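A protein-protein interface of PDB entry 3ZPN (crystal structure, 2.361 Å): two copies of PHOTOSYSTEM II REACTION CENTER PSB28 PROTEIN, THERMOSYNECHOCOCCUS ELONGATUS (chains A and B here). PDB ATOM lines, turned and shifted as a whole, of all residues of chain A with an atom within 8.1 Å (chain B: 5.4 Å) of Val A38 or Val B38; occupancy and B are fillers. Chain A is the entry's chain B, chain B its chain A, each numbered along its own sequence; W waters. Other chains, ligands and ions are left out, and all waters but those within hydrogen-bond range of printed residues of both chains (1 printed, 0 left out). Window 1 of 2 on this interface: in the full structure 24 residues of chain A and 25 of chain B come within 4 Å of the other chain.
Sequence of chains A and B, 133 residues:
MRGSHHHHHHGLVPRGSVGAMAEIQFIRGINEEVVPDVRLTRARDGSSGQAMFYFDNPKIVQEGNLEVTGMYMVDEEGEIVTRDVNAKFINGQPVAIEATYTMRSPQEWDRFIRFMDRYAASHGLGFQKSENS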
ATOM      1  N   ILE A  24       6.910  13.249  -8.882  1.00  0.00           N
ATOM      2  CA  ILE A  24       5.560  13.669  -8.581  1.00  0.00           C
ATOM      3  C   ILE A  24       5.149  13.089  -7.233  1.00  0.00           C
ATOM      4  O   ILE A  24       5.373  11.906  -6.976  1.00  0.00           O
ATOM      5  CB  ILE A  24       4.577  13.190  -9.658  1.00  0.00           C
ATOM      6  CG1 ILE A  24       4.905  13.849 -10.995  1.00  0.00           C
ATOM      7  CG2 ILE A  24       3.106  13.479  -9.226  1.00  0.00           C
ATOM      8  CD1 ILE A  24       4.076  13.337 -12.140  1.00  0.00           C
ATOM      9  N   VAL A  35       3.601   5.791 -12.869  1.00  0.00           N
ATOM     10  CA  VAL A  35       3.771   6.823 -13.881  1.00  0.00           C
ATOM     11  C   VAL A  35       2.421   7.100 -14.528  1.00  0.00           C
ATOM     12  O   VAL A  35       1.731   6.162 -14.931  1.00  0.00           O
ATOM     13  CB  VAL A  35       4.754   6.393 -14.980  1.00  0.00           C
ATOM     14  CG1 VAL A  35       4.817   7.454 -16.074  1.00  0.00           C
ATOM     15  CG2 VAL A  35       6.116   6.129 -14.403  1.00  0.00           C
ATOM     16  N   PRO A  36       2.012   8.376 -14.588  1.00  0.00           N
ATOM     17  CA  PRO A  36       0.710   8.751 -15.148  1.00  0.00           C
ATOM     18  C   PRO A  36       0.682   8.778 -16.679  1.00  0.00           C
ATOM     19  O   PRO A  36       1.744   8.782 -17.303  1.00  0.00           O
ATOM     20  CB  PRO A  36       0.481  10.163 -14.579  1.00  0.00           C
ATOM     21  CG  PRO A  36       1.830  10.696 -14.390  1.00  0.00           C
ATOM     22  CD  PRO A  36       2.704   9.526 -13.990  1.00  0.00           C
ATOM     23  N   ASP A  37      -0.511   8.722 -17.269  1.00  0.00           N
ATOM     24  CA  ASP A  37      -0.696   9.185 -18.646  1.00  0.00           C
ATOM     25  C   ASP A  37      -0.734  10.712 -18.606  1.00  0.00           C
ATOM     26  O   ASP A  37      -1.314  11.303 -17.708  1.00  0.00           O
ATOM     27  CB  ASP A  37      -2.001   8.664 -19.237  1.00  0.00           C
ATOM     28  CG  ASP A  37      -2.061   7.139 -19.244  1.00  0.00           C
ATOM     29  OD1 ASP A  37      -0.983   6.497 -19.126  1.00  0.00           O
ATOM     30  OD2 ASP A  37      -3.187   6.588 -19.343  1.00  0.00           O
ATOM     31  N   VAL A  38      -0.111  11.361 -19.569  1.00  0.00           N
ATOM     32  CA  VAL A  38      -0.062  12.803 -19.521  1.00  0.00           C
ATOM     33  C   VAL A  38      -0.633  13.345 -20.823  1.00  0.00           C
ATOM     34  O   VAL A  38      -0.253  12.915 -21.913  1.00  0.00           O
ATOM     35  CB  VAL A  38       1.382  13.329 -19.311  1.00  0.00           C
ATOM     36  CG1 VAL A  38       1.367  14.834 -19.099  1.00  0.00           C
ATOM     37  CG2 VAL A  38       2.019  12.659 -18.116  1.00  0.00           C
ATOM     38  N   ARG A  39      -1.583  14.255 -20.706  1.00  0.00           N
ATOM     39  CA  ARG A  39      -2.130  14.930 -21.868  1.00  0.00           C
ATOM     40  C   ARG A  39      -1.828  16.435 -21.811  1.00  0.00           C
ATOM     41  O   ARG A  39      -2.023  17.093 -20.788  1.00  0.00           O
ATOM     42  CB  ARG A  39      -3.624  14.675 -21.970  1.00  0.00           C
ATOM     43  CG  ARG A  39      -4.313  15.375 -23.095  1.00  0.00           C
ATOM     44  CD  ARG A  39      -5.664  14.723 -23.344  1.00  0.00           C
ATOM     45  NE  ARG A  39      -6.579  15.618 -24.037  1.00  0.00           N
ATOM     46  CZ  ARG A  39      -7.357  16.503 -23.416  1.00  0.00           C
ATOM     47  NH1 ARG A  39      -7.319  16.606 -22.085  1.00  0.00           N
ATOM     48  NH2 ARG A  39      -8.174  17.285 -24.123  1.00  0.00           N
ATOM     49  N   LEU A  40      -1.311  16.964 -22.910  1.00  0.00           N
ATOM     50  CA  LEU A  40      -0.901  18.353 -22.951  1.00  0.00           C
ATOM     51  C   LEU A  40      -1.686  19.081 -24.039  1.00  0.00           C
ATOM     52  O   LEU A  40      -1.732  18.649 -25.181  1.00  0.00           O
ATOM     53  CB  LEU A  40       0.607  18.435 -23.187  1.00  0.00           C
ATOM     54  CG  LEU A  40       1.248  19.826 -23.203  1.00  0.00           C
ATOM     55  CD1 LEU A  40       1.048  20.589 -21.896  1.00  0.00           C
ATOM     56  CD2 LEU A  40       2.731  19.703 -23.519  1.00  0.00           C
ATOM     57  N   THR A  41      -2.342  20.163 -23.658  1.00  0.00           N
ATOM     58  CA  THR A  41      -3.103  20.946 -24.611  1.00  0.00           C
ATOM     59  C   THR A  41      -2.664  22.397 -24.569  1.00  0.00           C
ATOM     60  O   THR A  41      -2.191  22.875 -23.550  1.00  0.00           O
ATOM     61  CB  THR A  41      -4.605  20.876 -24.320  1.00  0.00           C
ATOM     62  OG1 THR A  41      -4.830  21.278 -22.967  1.00  0.00           O
ATOM     63  CG2 THR A  41      -5.103  19.444 -24.520  1.00  0.00           C
ATOM     64  N   ARG A  42      -2.914  23.115 -25.654  1.00  0.00           N
ATOM     65  CA  ARG A  42      -2.583  24.530 -25.758  1.00  0.00           C
ATOM     66  C   ARG A  42      -3.826  25.219 -26.341  1.00  0.00           C
ATOM     67  O   ARG A  42      -4.454  24.709 -27.270  1.00  0.00           O
ATOM     68  CB  ARG A  42      -1.374  24.713 -26.672  1.00  0.00           C
ATOM     69  CG  ARG A  42      -0.874  26.149 -26.862  1.00  0.00           C
ATOM     70  CD  ARG A  42       0.238  26.164 -27.914  1.00  0.00           C
ATOM     71  NE  ARG A  42       0.806  27.485 -28.129  1.00  0.00           N
ATOM     72  CZ  ARG A  42       0.413  28.345 -29.053  1.00  0.00           C
ATOM     73  NH1 ARG A  42      -0.541  28.026 -29.903  1.00  0.00           N
ATOM     74  NH2 ARG A  42       1.013  29.520 -29.147  1.00  0.00           N
ATOM     75  N   GLN A  50      -2.941  23.424 -20.714  1.00  0.00           N
ATOM     76  CA  GLN A  50      -3.329  22.487 -19.658  1.00  0.00           C
ATOM     77  C   GLN A  50      -2.538  21.176 -19.719  1.00  0.00           C
ATOM     78  O   GLN A  50      -2.379  20.559 -20.775  1.00  0.00           O
ATOM     79  CB  GLN A  50      -4.814  22.145 -19.741  1.00  0.00           C
ATOM     80  CG  GLN A  50      -5.761  23.174 -19.151  1.00  0.00           C
ATOM     81  CD  GLN A  50      -7.113  22.581 -18.721  1.00  0.00           C
ATOM     82  OE1 GLN A  50      -7.574  21.557 -19.258  1.00  0.00           O
ATOM     83  NE2 GLN A  50      -7.770  23.257 -17.773  1.00  0.00           N
ATOM     84  N   ALA A  51      -2.114  20.714 -18.559  1.00  0.00           N
ATOM     85  CA  ALA A  51      -1.538  19.390 -18.468  1.00  0.00           C
ATOM     86  C   ALA A  51      -2.460  18.524 -17.609  1.00  0.00           C
ATOM     87  O   ALA A  51      -2.803  18.891 -16.481  1.00  0.00           O
ATOM     88  CB  ALA A  51      -0.125  19.447 -17.860  1.00  0.00           C
ATOM     89  N   MET A  52      -2.847  17.372 -18.142  1.00  0.00           N
ATOM     90  CA  MET A  52      -3.724  16.462 -17.431  1.00  0.00           C
ATOM     91  C   MET A  52      -2.975  15.166 -17.121  1.00  0.00           C
ATOM     92  O   MET A  52      -2.302  14.616 -17.978  1.00  0.00           O
ATOM     93  CB  MET A  52      -4.980  16.185 -18.265  1.00  0.00           C
ATOM     94  CG  MET A  52      -6.123  17.142 -18.074  1.00  0.00           C
ATOM     95  SD  MET A  52      -6.910  17.746 -19.612  1.00  0.00           S
ATOM     96  CE  MET A  52      -5.525  18.639 -20.392  1.00  0.00           C
ATOM     97  N   PHE A  53      -3.101  14.675 -15.898  1.00  0.00           N
ATOM     98  CA  PHE A  53      -2.375  13.480 -15.452  1.00  0.00           C
ATOM     99  C   PHE A  53      -3.400  12.447 -15.034  1.00  0.00           C
ATOM    100  O   PHE A  53      -4.329  12.767 -14.285  1.00  0.00           O
ATOM    101  CB  PHE A  53      -1.472  13.787 -14.259  1.00  0.00           C
ATOM    102  CG  PHE A  53      -0.379  14.767 -14.553  1.00  0.00           C
ATOM    103  CD1 PHE A  53      -0.653  16.116 -14.727  1.00  0.00           C
ATOM    104  CD2 PHE A  53       0.942  14.347 -14.597  1.00  0.00           C
ATOM    105  CE1 PHE A  53       0.386  17.028 -14.985  1.00  0.00           C
ATOM    106  CE2 PHE A  53       1.969  15.237 -14.849  1.00  0.00           C
ATOM    107  CZ  PHE A  53       1.694  16.578 -15.044  1.00  0.00           C
ATOM    108  N   TYR A  54      -3.260  11.212 -15.505  1.00  0.00           N
ATOM    109  CA  TYR A  54      -4.188  10.197 -15.034  1.00  0.00           C
ATOM    110  C   TYR A  54      -3.391   9.027 -14.482  1.00  0.00           C
ATOM    111  O   TYR A  54      -2.629   8.388 -15.216  1.00  0.00           O
ATOM    112  CB  TYR A  54      -5.151   9.774 -16.154  1.00  0.00           C
ATOM    113  CG  TYR A  54      -6.333   8.974 -15.666  1.00  0.00           C
ATOM    114  CD1 TYR A  54      -6.246   7.591 -15.451  1.00  0.00           C
ATOM    115  CD2 TYR A  54      -7.547   9.603 -15.413  1.00  0.00           C
ATOM    116  CE1 TYR A  54      -7.349   6.864 -15.006  1.00  0.00           C
ATOM    117  CE2 TYR A  54      -8.644   8.896 -14.961  1.00  0.00           C
ATOM    118  CZ  TYR A  54      -8.546   7.524 -14.759  1.00  0.00           C
ATOM    119  OH  TYR A  54      -9.656   6.830 -14.321  1.00  0.00           O
ATOM    120  N   PHE A  55      -3.574   8.745 -13.193  1.00  0.00           N
ATOM    121  CA  PHE A  55      -2.829   7.681 -12.517  1.00  0.00           C
ATOM    122  C   PHE A  55      -3.714   6.470 -12.301  1.00  0.00           C
ATOM    123  O   PHE A  55      -4.771   6.579 -11.667  1.00  0.00           O
ATOM    124  CB  PHE A  55      -2.336   8.134 -11.152  1.00  0.00           C
ATOM    125  CG  PHE A  55      -1.299   9.201 -11.183  1.00  0.00           C
ATOM    126  CD1 PHE A  55      -1.644  10.517 -11.445  1.00  0.00           C
ATOM    127  CD2 PHE A  55       0.021   8.908 -10.835  1.00  0.00           C
ATOM    128  CE1 PHE A  55      -0.669  11.513 -11.434  1.00  0.00           C
ATOM    129  CE2 PHE A  55       0.998   9.887 -10.813  1.00  0.00           C
ATOM    130  CZ  PHE A  55       0.657  11.190 -11.107  1.00  0.00           C
ATOM    131  N   ALA A  99      -5.437  14.563 -12.255  1.00  0.00           N
ATOM    132  CA  ALA A  99      -4.995  15.892 -11.858  1.00  0.00           C
ATOM    133  C   ALA A  99      -4.878  16.787 -13.069  1.00  0.00           C
ATOM    134  O   ALA A  99      -4.383  16.373 -14.108  1.00  0.00           O
ATOM    135  CB  ALA A  99      -3.662  15.824 -11.136  1.00  0.00           C
ATOM    136  N   PHE A 112       6.897  24.642 -16.533  1.00  0.00           N
ATOM    137  CA  PHE A 112       6.325  23.309 -16.520  1.00  0.00           C
ATOM    138  C   PHE A 112       6.993  22.358 -17.477  1.00  0.00           C
ATOM    139  O   PHE A 112       7.137  21.170 -17.183  1.00  0.00           O
ATOM    140  CB  PHE A 112       4.839  23.316 -16.809  1.00  0.00           C
ATOM    141  CG  PHE A 112       4.288  21.943 -17.000  1.00  0.00           C
ATOM    142  CD1 PHE A 112       4.112  21.100 -15.909  1.00  0.00           C
ATOM    143  CD2 PHE A 112       3.955  21.485 -18.254  1.00  0.00           C
ATOM    144  CE1 PHE A 112       3.608  19.816 -16.062  1.00  0.00           C
ATOM    145  CE2 PHE A 112       3.439  20.197 -18.425  1.00  0.00           C
ATOM    146  CZ  PHE A 112       3.268  19.360 -17.316  1.00  0.00           C
ATOM    147  N   MET A 116       8.747  18.672 -16.802  1.00  0.00           N
ATOM    148  CA  MET A 116       8.300  17.503 -17.536  1.00  0.00           C
ATOM    149  C   MET A 116       9.440  16.801 -18.255  1.00  0.00           C
ATOM    150  O   MET A 116       9.469  15.573 -18.354  1.00  0.00           O
ATOM    151  CB  MET A 116       7.196  17.897 -18.517  1.00  0.00           C
ATOM    152  CG  MET A 116       6.248  16.767 -18.878  1.00  0.00           C
ATOM    153  SD  MET A 116       5.308  16.087 -17.500  1.00  0.00           S
ATOM    154  CE  MET A 116       5.586  14.347 -17.771  1.00  0.00           C
ATOM    155  N   TYR A 119      11.315  14.966 -15.730  1.00  0.00           N
ATOM    156  CA  TYR A 119      10.516  13.829 -15.292  1.00  0.00           C
ATOM    157  C   TYR A 119      10.499  12.691 -16.310  1.00  0.00           C
ATOM    158  O   TYR A 119      10.791  11.546 -15.959  1.00  0.00           O
ATOM    159  CB  TYR A 119       9.079  14.236 -14.938  1.00  0.00           C
ATOM    160  CG  TYR A 119       8.239  13.054 -14.491  1.00  0.00           C
ATOM    161  CD1 TYR A 119       8.236  12.645 -13.151  1.00  0.00           C
ATOM    162  CD2 TYR A 119       7.463  12.319 -15.406  1.00  0.00           C
ATOM    163  CE1 TYR A 119       7.478  11.538 -12.724  1.00  0.00           C
ATOM    164  CE2 TYR A 119       6.699  11.204 -14.984  1.00  0.00           C
ATOM    165  CZ  TYR A 119       6.708  10.834 -13.649  1.00  0.00           C
ATOM    166  OH  TYR A 119       5.957   9.761 -13.241  1.00  0.00           O
ATOM    167  N   ALA A 120      10.157  13.005 -17.559  1.00  0.00           N
ATOM    168  CA  ALA A 120      10.056  11.987 -18.613  1.00  0.00           C
ATOM    169  C   ALA A 120      11.401  11.315 -18.913  1.00  0.00           C
ATOM    170  O   ALA A 120      11.455  10.118 -19.247  1.00  0.00           O
ATOM    171  CB  ALA A 120       9.443  12.585 -19.900  1.00  0.00           C
ATOM    172  N   PRO B  36      -0.675  20.422 -32.051  1.00  0.00           N
ATOM    173  CA  PRO B  36      -1.569  19.308 -31.679  1.00  0.00           C
ATOM    174  C   PRO B  36      -1.858  19.213 -30.182  1.00  0.00           C
ATOM    175  O   PRO B  36      -1.119  19.796 -29.390  1.00  0.00           O
ATOM    176  CB  PRO B  36      -0.791  18.063 -32.128  1.00  0.00           C
ATOM    177  CG  PRO B  36       0.691  18.497 -32.001  1.00  0.00           C
ATOM    178  CD  PRO B  36       0.699  19.974 -32.370  1.00  0.00           C
ATOM    179  N   ASP B  37      -2.942  18.532 -29.810  1.00  0.00           N
ATOM    180  CA  ASP B  37      -3.066  17.987 -28.456  1.00  0.00           C
ATOM    181  C   ASP B  37      -2.176  16.750 -28.430  1.00  0.00           C
ATOM    182  O   ASP B  37      -2.195  15.966 -29.386  1.00  0.00           O
ATOM    183  CB  ASP B  37      -4.506  17.550 -28.144  1.00  0.00           C
ATOM    184  CG  ASP B  37      -5.512  18.691 -28.194  1.00  0.00           C
ATOM    185  OD1 ASP B  37      -5.122  19.870 -28.081  1.00  0.00           O
ATOM    186  OD2 ASP B  37      -6.713  18.394 -28.367  1.00  0.00           O
ATOM    187  N   VAL B  38      -1.429  16.541 -27.349  1.00  0.00           N
ATOM    188  CA  VAL B  38      -0.487  15.416 -27.278  1.00  0.00           C
ATOM    189  C   VAL B  38      -0.732  14.532 -26.073  1.00  0.00           C
ATOM    190  O   VAL B  38      -0.849  15.025 -24.964  1.00  0.00           O
ATOM    191  CB  VAL B  38       1.005  15.888 -27.236  1.00  0.00           C
ATOM    192  CG1 VAL B  38       1.953  14.695 -27.093  1.00  0.00           C
ATOM    193  CG2 VAL B  38       1.333  16.752 -28.455  1.00  0.00           C
ATOM    194  N   ARG B  39      -0.853  13.228 -26.287  1.00  0.00           N
ATOM    195  CA  ARG B  39      -0.996  12.336 -25.144  1.00  0.00           C
ATOM    196  C   ARG B  39       0.180  11.372 -25.072  1.00  0.00           C
ATOM    197  O   ARG B  39       0.537  10.714 -26.052  1.00  0.00           O
ATOM    198  CB  ARG B  39      -2.321  11.586 -25.180  1.00  0.00           C
ATOM    199  CG  ARG B  39      -2.609  10.847 -23.887  1.00  0.00           C
ATOM    200  CD  ARG B  39      -4.029  10.274 -23.873  1.00  0.00           C
ATOM    201  NE  ARG B  39      -4.161   9.002 -24.567  1.00  0.00           N
ATOM    202  CZ  ARG B  39      -4.327   7.838 -23.945  1.00  0.00           C
ATOM    203  NH1 ARG B  39      -4.428   7.803 -22.624  1.00  0.00           N
ATOM    204  NH2 ARG B  39      -4.436   6.716 -24.638  1.00  0.00           N
ATOM    205  N   LEU B  40       0.774  11.283 -23.896  1.00  0.00           N
ATOM    206  CA  LEU B  40       1.970  10.483 -23.723  1.00  0.00           C
ATOM    207  C   LEU B  40       1.693   9.365 -22.727  1.00  0.00           C
ATOM    208  O   LEU B  40       1.224   9.619 -21.606  1.00  0.00           O
ATOM    209  CB  LEU B  40       3.107  11.371 -23.240  1.00  0.00           C
ATOM    210  CG  LEU B  40       4.529  10.858 -23.331  1.00  0.00           C
ATOM    211  CD1 LEU B  40       5.380  12.000 -23.790  1.00  0.00           C
ATOM    212  CD2 LEU B  40       5.015  10.397 -21.980  1.00  0.00           C
ATOM    213  N   THR B  41       1.938   8.128 -23.155  1.00  0.00           N
ATOM    214  CA  THR B  41       1.744   6.974 -22.278  1.00  0.00           C
ATOM    215  C   THR B  41       3.003   6.122 -22.177  1.00  0.00           C
ATOM    216  O   THR B  41       3.884   6.180 -23.038  1.00  0.00           O
ATOM    217  CB  THR B  41       0.609   6.058 -22.745  1.00  0.00           C
ATOM    218  OG1 THR B  41       0.880   5.599 -24.080  1.00  0.00           O
ATOM    219  CG2 THR B  41      -0.730   6.781 -22.655  1.00  0.00           C
ATOM    220  N   ALA B  51       3.195   8.103 -28.054  1.00  0.00           N
ATOM    221  CA  ALA B  51       2.713   9.480 -28.136  1.00  0.00           C
ATOM    222  C   ALA B  51       1.644   9.570 -29.226  1.00  0.00           C
ATOM    223  O   ALA B  51       1.826   9.072 -30.338  1.00  0.00           O
ATOM    224  CB  ALA B  51       3.849  10.452 -28.410  1.00  0.00           C
ATOM    225  N   MET B  52       0.509  10.160 -28.873  1.00  0.00           N
ATOM    226  CA  MET B  52      -0.616  10.314 -29.785  1.00  0.00           C
ATOM    227  C   MET B  52      -0.920  11.777 -30.012  1.00  0.00           C
ATOM    228  O   MET B  52      -0.957  12.551 -29.063  1.00  0.00           O
ATOM    229  CB  MET B  52      -1.844   9.575 -29.249  1.00  0.00           C
ATOM    230  CG  MET B  52      -1.585   8.105 -28.964  1.00  0.00           C
ATOM    231  SD  MET B  52      -3.128   7.248 -28.671  1.00  0.00           S
ATOM    232  CE  MET B  52      -2.687   6.334 -27.201  1.00  0.00           C
ATOM    233  N   PHE B  53      -1.173  12.137 -31.264  1.00  0.00           N
ATOM    234  CA  PHE B  53      -1.292  13.536 -31.656  1.00  0.00           C
ATOM    235  C   PHE B  53      -2.641  13.812 -32.282  1.00  0.00           C
ATOM    236  O   PHE B  53      -3.097  13.071 -33.142  1.00  0.00           O
ATOM    237  CB  PHE B  53      -0.212  13.891 -32.668  1.00  0.00           C
ATOM    238  CG  PHE B  53       1.194  13.681 -32.163  1.00  0.00           C
ATOM    239  CD1 PHE B  53       1.729  12.403 -32.066  1.00  0.00           C
ATOM    240  CD2 PHE B  53       1.993  14.765 -31.809  1.00  0.00           C
ATOM    241  CE1 PHE B  53       3.028  12.206 -31.616  1.00  0.00           C
ATOM    242  CE2 PHE B  53       3.287  14.576 -31.366  1.00  0.00           C
ATOM    243  CZ  PHE B  53       3.807  13.292 -31.270  1.00  0.00           C
ATOM    244  N   TYR B  54      -3.278  14.886 -31.849  1.00  0.00           N
ATOM    245  CA  TYR B  54      -4.527  15.311 -32.453  1.00  0.00           C
ATOM    246  C   TYR B  54      -4.397  16.727 -32.961  1.00  0.00           C
ATOM    247  O   TYR B  54      -4.146  17.639 -32.190  1.00  0.00           O
ATOM    248  CB  TYR B  54      -5.710  15.206 -31.470  1.00  0.00           C
ATOM    249  CG  TYR B  54      -7.024  15.584 -32.118  1.00  0.00           C
ATOM    250  CD1 TYR B  54      -7.766  14.662 -32.845  1.00  0.00           C
ATOM    251  CD2 TYR B  54      -7.504  16.885 -32.035  1.00  0.00           C
ATOM    252  CE1 TYR B  54      -8.955  15.024 -33.461  1.00  0.00           C
ATOM    253  CE2 TYR B  54      -8.682  17.253 -32.638  1.00  0.00           C
ATOM    254  CZ  TYR B  54      -9.402  16.322 -33.352  1.00  0.00           C
ATOM    255  OH  TYR B  54     -10.576  16.699 -33.956  1.00  0.00           O
ATOM    256  N   MET B 116      10.450  16.568 -28.072  1.00  0.00           N
ATOM    257  CA  MET B 116       9.243  17.122 -27.474  1.00  0.00           C
ATOM    258  C   MET B 116       9.546  18.353 -26.599  1.00  0.00           C
ATOM    259  O   MET B 116       8.769  19.310 -26.585  1.00  0.00           O
ATOM    260  CB  MET B 116       8.513  16.035 -26.676  1.00  0.00           C
ATOM    261  CG  MET B 116       7.016  16.214 -26.510  1.00  0.00           C
ATOM    262  SD  MET B 116       6.108  16.193 -28.060  1.00  0.00           S
ATOM    263  CE  MET B 116       5.064  17.634 -27.847  1.00  0.00           C
HETATM  264  O   HOH W   1      -3.064  21.713 -28.045  1.00  0.00           O
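The guanidinium group (NH1) of Arg B39 lies within salt-bridge range of the side-chain carboxylate (OD2) of Asp A37 (3.7 Å). The backbone NH (N) of Leu B40 is in hydrogen-bond range of the backbone carbonyl oxygen (O) of Val A38, 2.8 Å away. The backbone carbonyl oxygen of Val B38 lies within hydrogen-bond range of the backbone NH of Leu A40.
N of Asp B37 is in hydrogen-bond range of O of Tyr B54 (2.8 Å). The backbone carbonyl oxygen (O) of Gln A50 is in hydrogen-bond range of the backbone NH (N) of Thr A41 (2.9 Å). SD of Met A52 is in hydrogen-bond range of NH1 of Arg A39 (2.8 Å). O of Asp A37 lies within hydrogen-bond range of N of Tyr A54, 2.9 Å away. The backbone NH (N) of Arg B39 is in hydrogen-bond range of the backbone carbonyl oxygen (O) of Met B52, 2.9 Å away.
Asp A37 touches Leu B40. OD1 of Asp A37 touches CG2 of Thr B41, at 3.5 Å. Val A38 touches Val B38 (O to O, 3.8 Å). CA of Arg B39 touches O of Val A38, at 3.4 Å. Arg A39 touches Val B38 (CA to O, 3.4 Å). Leu A40 touches Asp B37 (O to CA, 3.6 Å). CG2 of Thr A41 touches OD1 of Asp B37, 3.6 Å away.
Val A38 touches three residues of chain B. Val B38 touches three residues of chain A. Printed residues of chain A within 4 Å of Asp B37: Leu A40 (3.6 Å) and Thr A41 (3.6 Å). Printed residues of chain B within 4 Å of Arg A39: Val B38 (3.4 Å). Of the printed residues of chain B, Asp A37 touches Arg B39 (3.7 Å), Leu B40 (3.6 Å) and Thr B41 (3.5 Å). Printed residues of chain A within 4 Å of Arg B39: Asp A37 and Val A38. Printed residues of chain B within 4 Å of Thr A41: Asp B37. Tyr A119 touches none of the printed residues of chain B. Phe B53 touches none of the printed residues of chain A. The nearest residue of chain B that does not touch Val A38 is Thr B41 (5.2 Å).
Hydrophobic or aromatic side chains of chain B within 4 Å of the printed part of chain A: Leu B40. Along chain B the printed residues that touch a printed residue of chain A span positions 37 to 41. Of the 20 printed residues of chain A, 5 touch a printed residue of chain B. Among the printed residues, 10 pairs touch across the chains. Among the printed residues, Asp or Glu carboxylates within 4 Å of a Lys or Arg side-chain nitrogen of the other chain: Asp A37 with Arg B39.
Asp A37 touches Arg B39, but with the chains exchanged Arg A39 does not touch Asp B37 (4.6 Å). Asp A37 touches Leu B40, and with the chains exchanged Leu A40 touches Asp B37. Asp A37 touches Thr B41, and with the chains exchanged Thr A41 touches Asp B37. Val A38 touches Arg B39, and with the chains exchanged Arg A39 touches Val B38. Positions printed for both chains: 36, 37, 38, 39, 40, 41, 51, 52, 53, 54 and 116. Of the 10 pairs that touch across the chains among the printed residues, 9 have their exchanged pair printed and touching as well.
Water W1 lies within hydrogen-bond range of OD1 of Asp B37 (2.8 Å), N of Arg A42 (2.8 Å) and O of Pro B36 (3.0 Å).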
